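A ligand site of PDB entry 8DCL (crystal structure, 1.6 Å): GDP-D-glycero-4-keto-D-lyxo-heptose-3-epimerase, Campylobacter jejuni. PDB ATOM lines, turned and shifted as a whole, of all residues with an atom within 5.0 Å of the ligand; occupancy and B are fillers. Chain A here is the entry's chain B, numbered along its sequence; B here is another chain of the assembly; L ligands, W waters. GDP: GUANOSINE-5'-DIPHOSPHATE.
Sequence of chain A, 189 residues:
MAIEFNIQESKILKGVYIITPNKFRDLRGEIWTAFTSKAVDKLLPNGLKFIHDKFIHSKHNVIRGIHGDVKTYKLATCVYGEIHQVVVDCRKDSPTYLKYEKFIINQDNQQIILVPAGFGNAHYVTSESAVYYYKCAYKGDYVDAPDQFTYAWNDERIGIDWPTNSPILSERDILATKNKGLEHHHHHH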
ATOM      1  N   LYS A  54      16.370 -15.837   5.613  1.00  0.00           N
ATOM      2  CA  LYS A  54      15.663 -14.783   6.343  1.00  0.00           C
ATOM      3  C   LYS A  54      16.555 -14.252   7.451  1.00  0.00           C
ATOM      4  O   LYS A  54      17.371 -15.002   8.045  1.00  0.00           O
ATOM      5  CB  LYS A  54      14.372 -15.337   6.948  1.00  0.00           C
ATOM      6  CG  LYS A  54      13.355 -15.841   5.942  1.00  0.00           C
ATOM      7  CD  LYS A  54      12.024 -16.156   6.567  1.00  0.00           C
ATOM      8  CE  LYS A  54      11.275 -14.930   7.039  1.00  0.00           C
ATOM      9  NZ  LYS A  54       9.941 -15.204   7.663  1.00  0.00           N
ATOM     10  N   ILE A  56      16.154 -11.738  11.057  1.00  0.00           N
ATOM     11  CA  ILE A  56      15.329 -11.088  12.090  1.00  0.00           C
ATOM     12  C   ILE A  56      16.256 -10.314  13.008  1.00  0.00           C
ATOM     13  O   ILE A  56      17.003 -10.931  13.721  1.00  0.00           O
ATOM     14  CB  ILE A  56      14.469 -12.070  12.907  1.00  0.00           C
ATOM     15  CG1 ILE A  56      13.698 -13.050  12.047  1.00  0.00           C
ATOM     16  CG2 ILE A  56      13.517 -11.287  13.780  1.00  0.00           C
ATOM     17  CD1 ILE A  56      12.876 -14.059  12.859  1.00  0.00           C
ATOM     18  N   ARG A  64      10.533 -14.482  20.164  1.00  0.00           N
ATOM     19  CA  ARG A  64       9.731 -14.770  18.968  1.00  0.00           C
ATOM     20  C   ARG A  64       9.447 -16.259  18.942  1.00  0.00           C
ATOM     21  O   ARG A  64      10.358 -17.005  19.128  1.00  0.00           O
ATOM     22  CB  ARG A  64      10.442 -14.317  17.709  1.00  0.00           C
ATOM     23  CG  ARG A  64      10.769 -12.826  17.707  1.00  0.00           C
ATOM     24  CD  ARG A  64      11.146 -12.405  16.313  1.00  0.00           C
ATOM     25  NE  ARG A  64      11.446 -11.002  16.223  1.00  0.00           N
ATOM     26  CZ  ARG A  64      10.888 -10.125  15.409  1.00  0.00           C
ATOM     27  NH1 ARG A  64       9.876 -10.477  14.614  1.00  0.00           N
ATOM     28  NH2 ARG A  64      11.406  -8.913  15.385  1.00  0.00           N
ATOM     29  N   HIS A  67       6.819 -21.093  16.847  1.00  0.00           N
ATOM     30  CA  HIS A  67       6.192 -21.115  15.506  1.00  0.00           C
ATOM     31  C   HIS A  67       6.644 -22.361  14.736  1.00  0.00           C
ATOM     32  O   HIS A  67       7.834 -22.721  14.788  1.00  0.00           O
ATOM     33  CB  HIS A  67       6.578 -19.887  14.705  1.00  0.00           C
ATOM     34  CG  HIS A  67       6.155 -18.616  15.347  1.00  0.00           C
ATOM     35  ND1 HIS A  67       6.542 -17.389  14.866  1.00  0.00           N
ATOM     36  CD2 HIS A  67       5.396 -18.380  16.440  1.00  0.00           C
ATOM     37  CE1 HIS A  67       6.013 -16.442  15.621  1.00  0.00           C
ATOM     38  NE2 HIS A  67       5.338 -17.018  16.612  1.00  0.00           N
ATOM     39  N   TYR A 142       5.725 -20.774   0.520  1.00  0.00           N
ATOM     40  CA  TYR A 142       6.118 -20.385   1.898  1.00  0.00           C
ATOM     41  C   TYR A 142       4.863 -20.378   2.784  1.00  0.00           C
ATOM     42  O   TYR A 142       3.791 -19.868   2.380  1.00  0.00           O
ATOM     43  CB  TYR A 142       6.803 -19.021   1.849  1.00  0.00           C
ATOM     44  CG  TYR A 142       7.181 -18.525   3.199  1.00  0.00           C
ATOM     45  CD1 TYR A 142       8.278 -19.060   3.847  1.00  0.00           C
ATOM     46  CD2 TYR A 142       6.432 -17.539   3.855  1.00  0.00           C
ATOM     47  CE1 TYR A 142       8.621 -18.641   5.115  1.00  0.00           C
ATOM     48  CE2 TYR A 142       6.761 -17.131   5.138  1.00  0.00           C
ATOM     49  CZ  TYR A 142       7.859 -17.677   5.757  1.00  0.00           C
ATOM     50  OH  TYR A 142       8.228 -17.307   7.022  1.00  0.00           O
ATOM     51  N   ASP A 144       3.042 -18.820   5.561  1.00  0.00           N
ATOM     52  CA  ASP A 144       3.113 -17.565   6.344  1.00  0.00           C
ATOM     53  C   ASP A 144       2.361 -17.778   7.653  1.00  0.00           C
ATOM     54  O   ASP A 144       1.824 -18.909   7.892  1.00  0.00           O
ATOM     55  CB  ASP A 144       2.690 -16.316   5.549  1.00  0.00           C
ATOM     56  CG  ASP A 144       3.288 -15.006   6.075  1.00  0.00           C
ATOM     57  OD1 ASP A 144       4.145 -15.009   7.019  1.00  0.00           O
ATOM     58  OD2 ASP A 144       2.901 -13.951   5.532  1.00  0.00           O
ATOM     59  N   ALA A 145       2.413 -16.742   8.483  1.00  0.00           N
ATOM     60  CA  ALA A 145       2.071 -16.797   9.922  1.00  0.00           C
ATOM     61  C   ALA A 145       0.662 -17.344  10.084  1.00  0.00           C
ATOM     62  O   ALA A 145       0.442 -18.249  10.892  1.00  0.00           O
ATOM     63  CB  ALA A 145       2.266 -15.431  10.547  1.00  0.00           C
ATOM     64  N   GLN A 148       0.622 -21.207  10.032  1.00  0.00           N
ATOM     65  CA  GLN A 148       1.534 -21.837  11.005  1.00  0.00           C
ATOM     66  C   GLN A 148       0.770 -22.162  12.298  1.00  0.00           C
ATOM     67  O   GLN A 148      -0.225 -21.478  12.574  1.00  0.00           O
ATOM     68  CB  GLN A 148       2.682 -20.890  11.331  1.00  0.00           C
ATOM     69  CG  GLN A 148       3.559 -20.581  10.127  1.00  0.00           C
ATOM     70  CD  GLN A 148       4.608 -19.542  10.439  1.00  0.00           C
ATOM     71  OE1 GLN A 148       4.898 -19.233  11.606  1.00  0.00           O
ATOM     72  NE2 GLN A 148       5.207 -18.983   9.412  1.00  0.00           N
ATOM     73  N   SER A 170       4.811 -10.116  20.181  1.00  0.00           N
ATOM     74  CA  SER A 170       3.735  -9.759  19.218  1.00  0.00           C
ATOM     75  C   SER A 170       2.371 -10.172  19.749  1.00  0.00           C
ATOM     76  O   SER A 170       2.264 -11.068  20.560  1.00  0.00           O
ATOM     77  CB  SER A 170       3.950 -10.411  17.878  1.00  0.00           C
ATOM     78  OG  SER A 170       3.906 -11.833  18.004  1.00  0.00           O
ATOM     79  N   ARG A 172       0.322 -12.072  17.976  1.00  0.00           N
ATOM     80  CA  ARG A 172       0.255 -13.538  17.700  1.00  0.00           C
ATOM     81  C   ARG A 172       0.746 -14.316  18.925  1.00  0.00           C
ATOM     82  O   ARG A 172       0.109 -15.304  19.351  1.00  0.00           O
ATOM     83  CB  ARG A 172       1.057 -13.911  16.446  1.00  0.00           C
ATOM     84  CG  ARG A 172       1.161 -15.405  16.190  1.00  0.00           C
ATOM     85  CD  ARG A 172       2.025 -15.660  14.974  1.00  0.00           C
ATOM     86  NE  ARG A 172       2.277 -17.084  14.860  1.00  0.00           N
ATOM     87  CZ  ARG A 172       3.037 -17.663  13.935  1.00  0.00           C
ATOM     88  NH1 ARG A 172       3.143 -18.979  13.960  1.00  0.00           N
ATOM     89  NH2 ARG A 172       3.685 -16.943  13.021  1.00  0.00           N
ATOM     90  N   ASP A 173       1.895 -13.909  19.458  1.00  0.00           N
ATOM     91  CA  ASP A 173       2.601 -14.734  20.458  1.00  0.00           C
ATOM     92  C   ASP A 173       1.928 -14.507  21.815  1.00  0.00           C
ATOM     93  O   ASP A 173       2.086 -15.369  22.703  1.00  0.00           O
ATOM     94  CB  ASP A 173       4.097 -14.435  20.411  1.00  0.00           C
ATOM     95  CG  ASP A 173       4.749 -14.979  19.169  1.00  0.00           C
ATOM     96  OD1 ASP A 173       4.032 -15.669  18.387  1.00  0.00           O
ATOM     97  OD2 ASP A 173       5.938 -14.683  18.931  1.00  0.00           O
ATOM     98  N   ALA B   2       3.297  -9.574   2.314  1.00  0.00           N
ATOM     99  CA  ALA B   2       3.907 -10.622   1.453  1.00  0.00           C
ATOM    100  C   ALA B   2       5.430 -10.391   1.390  1.00  0.00           C
ATOM    101  O   ALA B   2       5.851  -9.264   1.595  1.00  0.00           O
ATOM    102  CB  ALA B   2       3.304 -10.574   0.081  1.00  0.00           C
ATOM    103  N   ILE B   3       6.203 -11.442   1.149  1.00  0.00           N
ATOM    104  CA  ILE B   3       7.655 -11.321   0.849  1.00  0.00           C
ATOM    105  C   ILE B   3       7.817 -10.777  -0.579  1.00  0.00           C
ATOM    106  O   ILE B   3       7.346 -11.470  -1.552  1.00  0.00           O
ATOM    107  CB  ILE B   3       8.350 -12.676   1.013  1.00  0.00           C
ATOM    108  CG1 ILE B   3       8.308 -13.139   2.468  1.00  0.00           C
ATOM    109  CG2 ILE B   3       9.770 -12.623   0.447  1.00  0.00           C
ATOM    110  CD1 ILE B   3       8.746 -14.581   2.694  1.00  0.00           C
ATOM    111  N   ASN B  22      11.369  -6.134   0.844  1.00  0.00           N
ATOM    112  CA  ASN B  22      10.547  -5.416   1.838  1.00  0.00           C
ATOM    113  C   ASN B  22      10.854  -5.966   3.237  1.00  0.00           C
ATOM    114  O   ASN B  22      11.572  -6.960   3.360  1.00  0.00           O
ATOM    115  CB  ASN B  22       9.081  -5.417   1.430  1.00  0.00           C
ATOM    116  CG  ASN B  22       8.431  -6.769   1.472  1.00  0.00           C
ATOM    117  OD1 ASN B  22       9.119  -7.801   1.490  1.00  0.00           O
ATOM    118  ND2 ASN B  22       7.099  -6.780   1.436  1.00  0.00           N
ATOM    119  N   LYS B  23      10.369  -5.301   4.278  1.00  0.00           N
ATOM    120  CA  LYS B  23      10.567  -5.729   5.681  1.00  0.00           C
ATOM    121  C   LYS B  23       9.255  -5.591   6.467  1.00  0.00           C
ATOM    122  O   LYS B  23       8.433  -4.740   6.086  1.00  0.00           O
ATOM    123  CB  LYS B  23      11.621  -4.869   6.358  1.00  0.00           C
ATOM    124  CG  LYS B  23      12.966  -4.799   5.654  1.00  0.00           C
ATOM    125  CD  LYS B  23      13.997  -4.269   6.545  1.00  0.00           C
ATOM    126  CE  LYS B  23      15.364  -4.334   5.920  1.00  0.00           C
ATOM    127  NZ  LYS B  23      16.387  -3.784   6.832  1.00  0.00           N
ATOM    128  N   PHE B  24       9.028  -6.456   7.443  1.00  0.00           N
ATOM    129  CA  PHE B  24       7.954  -6.259   8.437  1.00  0.00           C
ATOM    130  C   PHE B  24       8.626  -5.677   9.678  1.00  0.00           C
ATOM    131  O   PHE B  24       9.534  -6.328  10.284  1.00  0.00           O
ATOM    132  CB  PHE B  24       7.224  -7.562   8.730  1.00  0.00           C
ATOM    133  CG  PHE B  24       6.157  -7.381   9.789  1.00  0.00           C
ATOM    134  CD1 PHE B  24       4.908  -6.900   9.459  1.00  0.00           C
ATOM    135  CD2 PHE B  24       6.445  -7.656  11.115  1.00  0.00           C
ATOM    136  CE1 PHE B  24       3.954  -6.685  10.434  1.00  0.00           C
ATOM    137  CE2 PHE B  24       5.491  -7.440  12.104  1.00  0.00           C
ATOM    138  CZ  PHE B  24       4.243  -6.970  11.761  1.00  0.00           C
ATOM    139  N   ARG B  28       9.189  -5.180  18.054  1.00  0.00           N
ATOM    140  CA  ARG B  28      10.274  -6.124  18.418  1.00  0.00           C
ATOM    141  C   ARG B  28      11.528  -5.848  17.566  1.00  0.00           C
ATOM    142  O   ARG B  28      12.600  -6.267  17.972  1.00  0.00           O
ATOM    143  CB  ARG B  28       9.864  -7.573  18.189  1.00  0.00           C
ATOM    144  CG  ARG B  28       8.674  -8.036  19.032  1.00  0.00           C
ATOM    145  CD  ARG B  28       8.148  -9.368  18.538  1.00  0.00           C
ATOM    146  NE  ARG B  28       7.548  -9.287  17.213  1.00  0.00           N
ATOM    147  CZ  ARG B  28       7.197 -10.330  16.460  1.00  0.00           C
ATOM    148  NH1 ARG B  28       7.408 -11.565  16.902  1.00  0.00           N
ATOM    149  NH2 ARG B  28       6.717 -10.164  15.234  1.00  0.00           N
ATOM    150  N   ILE B  31      11.757  -8.166  10.374  1.00  0.00           N
ATOM    151  CA  ILE B  31      11.907  -9.479   9.706  1.00  0.00           C
ATOM    152  C   ILE B  31      11.986  -9.217   8.199  1.00  0.00           C
ATOM    153  O   ILE B  31      11.166  -8.434   7.673  1.00  0.00           O
ATOM    154  CB  ILE B  31      10.687 -10.390   9.928  1.00  0.00           C
ATOM    155  CG1 ILE B  31      10.149 -10.461  11.348  1.00  0.00           C
ATOM    156  CG2 ILE B  31      10.990 -11.785   9.375  1.00  0.00           C
ATOM    157  CD1 ILE B  31       8.734 -10.986  11.374  1.00  0.00           C
ATOM    158  N   TRP B  32      12.876  -9.903   7.510  1.00  0.00           N
ATOM    159  CA  TRP B  32      12.943  -9.770   6.045  1.00  0.00           C
ATOM    160  C   TRP B  32      13.624 -10.989   5.429  1.00  0.00           C
ATOM    161  O   TRP B  32      14.319 -11.761   6.142  1.00  0.00           O
ATOM    162  CB  TRP B  32      13.627  -8.468   5.617  1.00  0.00           C
ATOM    163  CG  TRP B  32      14.994  -8.242   6.216  1.00  0.00           C
ATOM    164  CD1 TRP B  32      15.310  -7.836   7.470  1.00  0.00           C
ATOM    165  CD2 TRP B  32      16.241  -8.389   5.521  1.00  0.00           C
ATOM    166  NE1 TRP B  32      16.663  -7.667   7.604  1.00  0.00           N
ATOM    167  CE2 TRP B  32      17.266  -8.060   6.445  1.00  0.00           C
ATOM    168  CE3 TRP B  32      16.599  -8.788   4.221  1.00  0.00           C
ATOM    169  CZ2 TRP B  32      18.608  -8.060   6.085  1.00  0.00           C
ATOM    170  CZ3 TRP B  32      17.924  -8.749   3.872  1.00  0.00           C
ATOM    171  CH2 TRP B  32      18.905  -8.403   4.794  1.00  0.00           C
ATOM    172  N   THR B  33      13.340 -11.163   4.155  1.00  0.00           N
ATOM    173  CA  THR B  33      13.876 -12.265   3.330  1.00  0.00           C
ATOM    174  C   THR B  33      14.980 -11.680   2.443  1.00  0.00           C
ATOM    175  O   THR B  33      14.749 -10.738   1.656  1.00  0.00           O
ATOM    176  CB  THR B  33      12.776 -12.946   2.495  1.00  0.00           C
ATOM    177  OG1 THR B  33      11.895 -13.582   3.426  1.00  0.00           O
ATOM    178  CG2 THR B  33      13.329 -13.946   1.502  1.00  0.00           C
HETATM  179  PB  GDP L   1       7.779 -13.807  14.066  1.00  0.00           P
HETATM  180  O1B GDP L   1       9.119 -13.146  14.052  1.00  0.00           O
HETATM  181  O2B GDP L   1       6.819 -13.374  15.171  1.00  0.00           O
HETATM  182  O3B GDP L   1       7.926 -15.299  13.783  1.00  0.00           O
HETATM  183  O3A GDP L   1       7.005 -13.215  12.773  1.00  0.00           O
HETATM  184  PA  GDP L   1       5.680 -13.909  12.194  1.00  0.00           P
HETATM  185  O1A GDP L   1       6.054 -15.106  11.313  1.00  0.00           O
HETATM  186  O2A GDP L   1       4.682 -13.908  13.335  1.00  0.00           O
HETATM  187  O5' GDP L   1       5.321 -12.698  11.176  1.00  0.00           O
HETATM  188  C5' GDP L   1       5.076 -11.392  11.671  1.00  0.00           C
HETATM  189  C4' GDP L   1       4.743 -10.552  10.455  1.00  0.00           C
HETATM  190  O4' GDP L   1       5.854 -10.422   9.521  1.00  0.00           O
HETATM  191  C3' GDP L   1       3.644 -11.269   9.692  1.00  0.00           C
HETATM  192  O3' GDP L   1       2.705 -10.323   9.189  1.00  0.00           O
HETATM  193  C2' GDP L   1       4.330 -11.899   8.484  1.00  0.00           C
HETATM  194  O2' GDP L   1       3.565 -11.914   7.274  1.00  0.00           O
HETATM  195  C1' GDP L   1       5.453 -10.915   8.248  1.00  0.00           C
HETATM  196  N9  GDP L   1       6.668 -11.538   7.713  1.00  0.00           N
HETATM  197  C8  GDP L   1       7.214 -12.688   8.145  1.00  0.00           C
HETATM  198  N7  GDP L   1       8.322 -12.949   7.403  1.00  0.00           N
HETATM  199  C5  GDP L   1       8.529 -11.949   6.525  1.00  0.00           C
HETATM  200  C6  GDP L   1       9.504 -11.593   5.498  1.00  0.00           C
HETATM  201  O6  GDP L   1      10.487 -12.334   5.310  1.00  0.00           O
HETATM  202  N1  GDP L   1       9.313 -10.451   4.814  1.00  0.00           N
HETATM  203  C2  GDP L   1       8.218  -9.645   5.059  1.00  0.00           C
HETATM  204  N2  GDP L   1       8.037  -8.534   4.342  1.00  0.00           N
HETATM  205  N3  GDP L   1       7.260  -9.924   5.990  1.00  0.00           N
HETATM  206  C4  GDP L   1       7.397 -11.026   6.749  1.00  0.00           C
HETATM  207  O   HOH W   1       2.438  -9.104   6.948  1.00  0.00           O
HETATM  208  O   HOH W   2       5.860  -6.769   4.661  1.00  0.00           O
HETATM  209  O   HOH W   3       6.053 -16.050   8.304  1.00  0.00           O
HETATM  210  O   HOH W   4       2.231 -12.841  13.061  1.00  0.00           O
HETATM  211  O   HOH W   5       1.412  -9.172  11.351  1.00  0.00           O
HETATM  212  O   HOH W   6      11.142  -9.578   2.925  1.00  0.00           O
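NZ of Lys 54 is in hydrogen-bond range of OH of Tyr 142, 2.8 Å away.
NE2 of His 67 sits at hydrogen-bond distance from OD1 of Asp 173 (2.6 Å).
The side-chain amide oxygen (OE1) of Gln 148 is in hydrogen-bond range of the guanidinium group (NH1) of Arg 172.
ND2 of Asn 22 of chain B lies within hydrogen-bond range of O of Ala 2 of chain B, at 2.8 Å.
The backbone carbonyl oxygen (O) of Phe 24 of chain B lies within hydrogen-bond range of the backbone NH (N) of Ile 31 of chain B, at 2.9 Å.
A ring nitrogen (ND1) of His 67 lies within hydrogen-bond range of the guanidinium group (NH2) of Arg 172, at 3.4 Å.
N7 of the ligand lies within hydrogen-bond range of NZ of Lys 54, 2.8 Å away.
An oxygen (O6) of the ligand sits at hydrogen-bond distance from the backbone NH of Thr 33 of chain B (3.3 Å).
The guanidinium group of Arg 172 is in salt-bridge range of an oxygen (O2A) of the ligand (3.2 Å).
An oxygen (O3B) of the ligand lies within hydrogen-bond range of a ring nitrogen (ND1) of His 67 (2.7 Å).
An oxygen (O1B) of the ligand lies within salt-bridge range of the guanidinium group (NH1) of Arg 64 (2.8 Å).
The side-chain carboxylate of Asp 144 is in hydrogen-bond range of an oxygen (O2') of the ligand.
The side-chain amide oxygen (OD1) of Asn 22 of chain B lies within hydrogen-bond range of a nitrogen (N2) of the ligand (3.1 Å).
The side-chain hydroxyl of Thr 33 of chain B is in hydrogen-bond range of an oxygen (O6) of the ligand, at 2.7 Å.
The guanidinium group (NH1) of Arg 28 of chain B lies within salt-bridge range of an oxygen (O2B) of the ligand, at 2.6 Å.
Water W6 lies within hydrogen-bond range of O of Asn 22 of chain B (2.7 Å), N1 of the ligand (2.8 Å) and N of Thr 33 of chain B (3.0 Å).
Water W2 bridges N2 of the ligand (2.8 Å) and ND2 of Asn 22 of chain B (3.5 Å).
Water W3 lies within hydrogen-bond range of the side-chain carboxylate (OD1) of Asp 144 (2.5 Å), the side-chain hydroxyl (OH) of Tyr 142 (2.8 Å), an oxygen (O1A) of the ligand (3.2 Å) and the side-chain amide nitrogen (NE2) of Gln 148 (3.2 Å).
CB of Ala 145 touches O1A of the ligand, 3.9 Å away.
Ala 2 of chain B touches the ligand.
Ile 3 of chain B touches the ligand (CG1 to C6, 3.6 Å).
C of Lys 23 of chain B touches N2 of the ligand (3.8 Å).
CG of Phe 24 of chain B touches O4' of the ligand, at 3.1 Å.
CD1 of Ile 31 of chain B touches O3A of the ligand, at 3.1 Å.
Trp 32 of chain B touches the ligand.
Hydrophobic or aromatic side chains within 4 Å of the ligand: His 67, Ala 145, Ile 3 of chain B, Phe 24 of chain B and Ile 31 of chain B.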
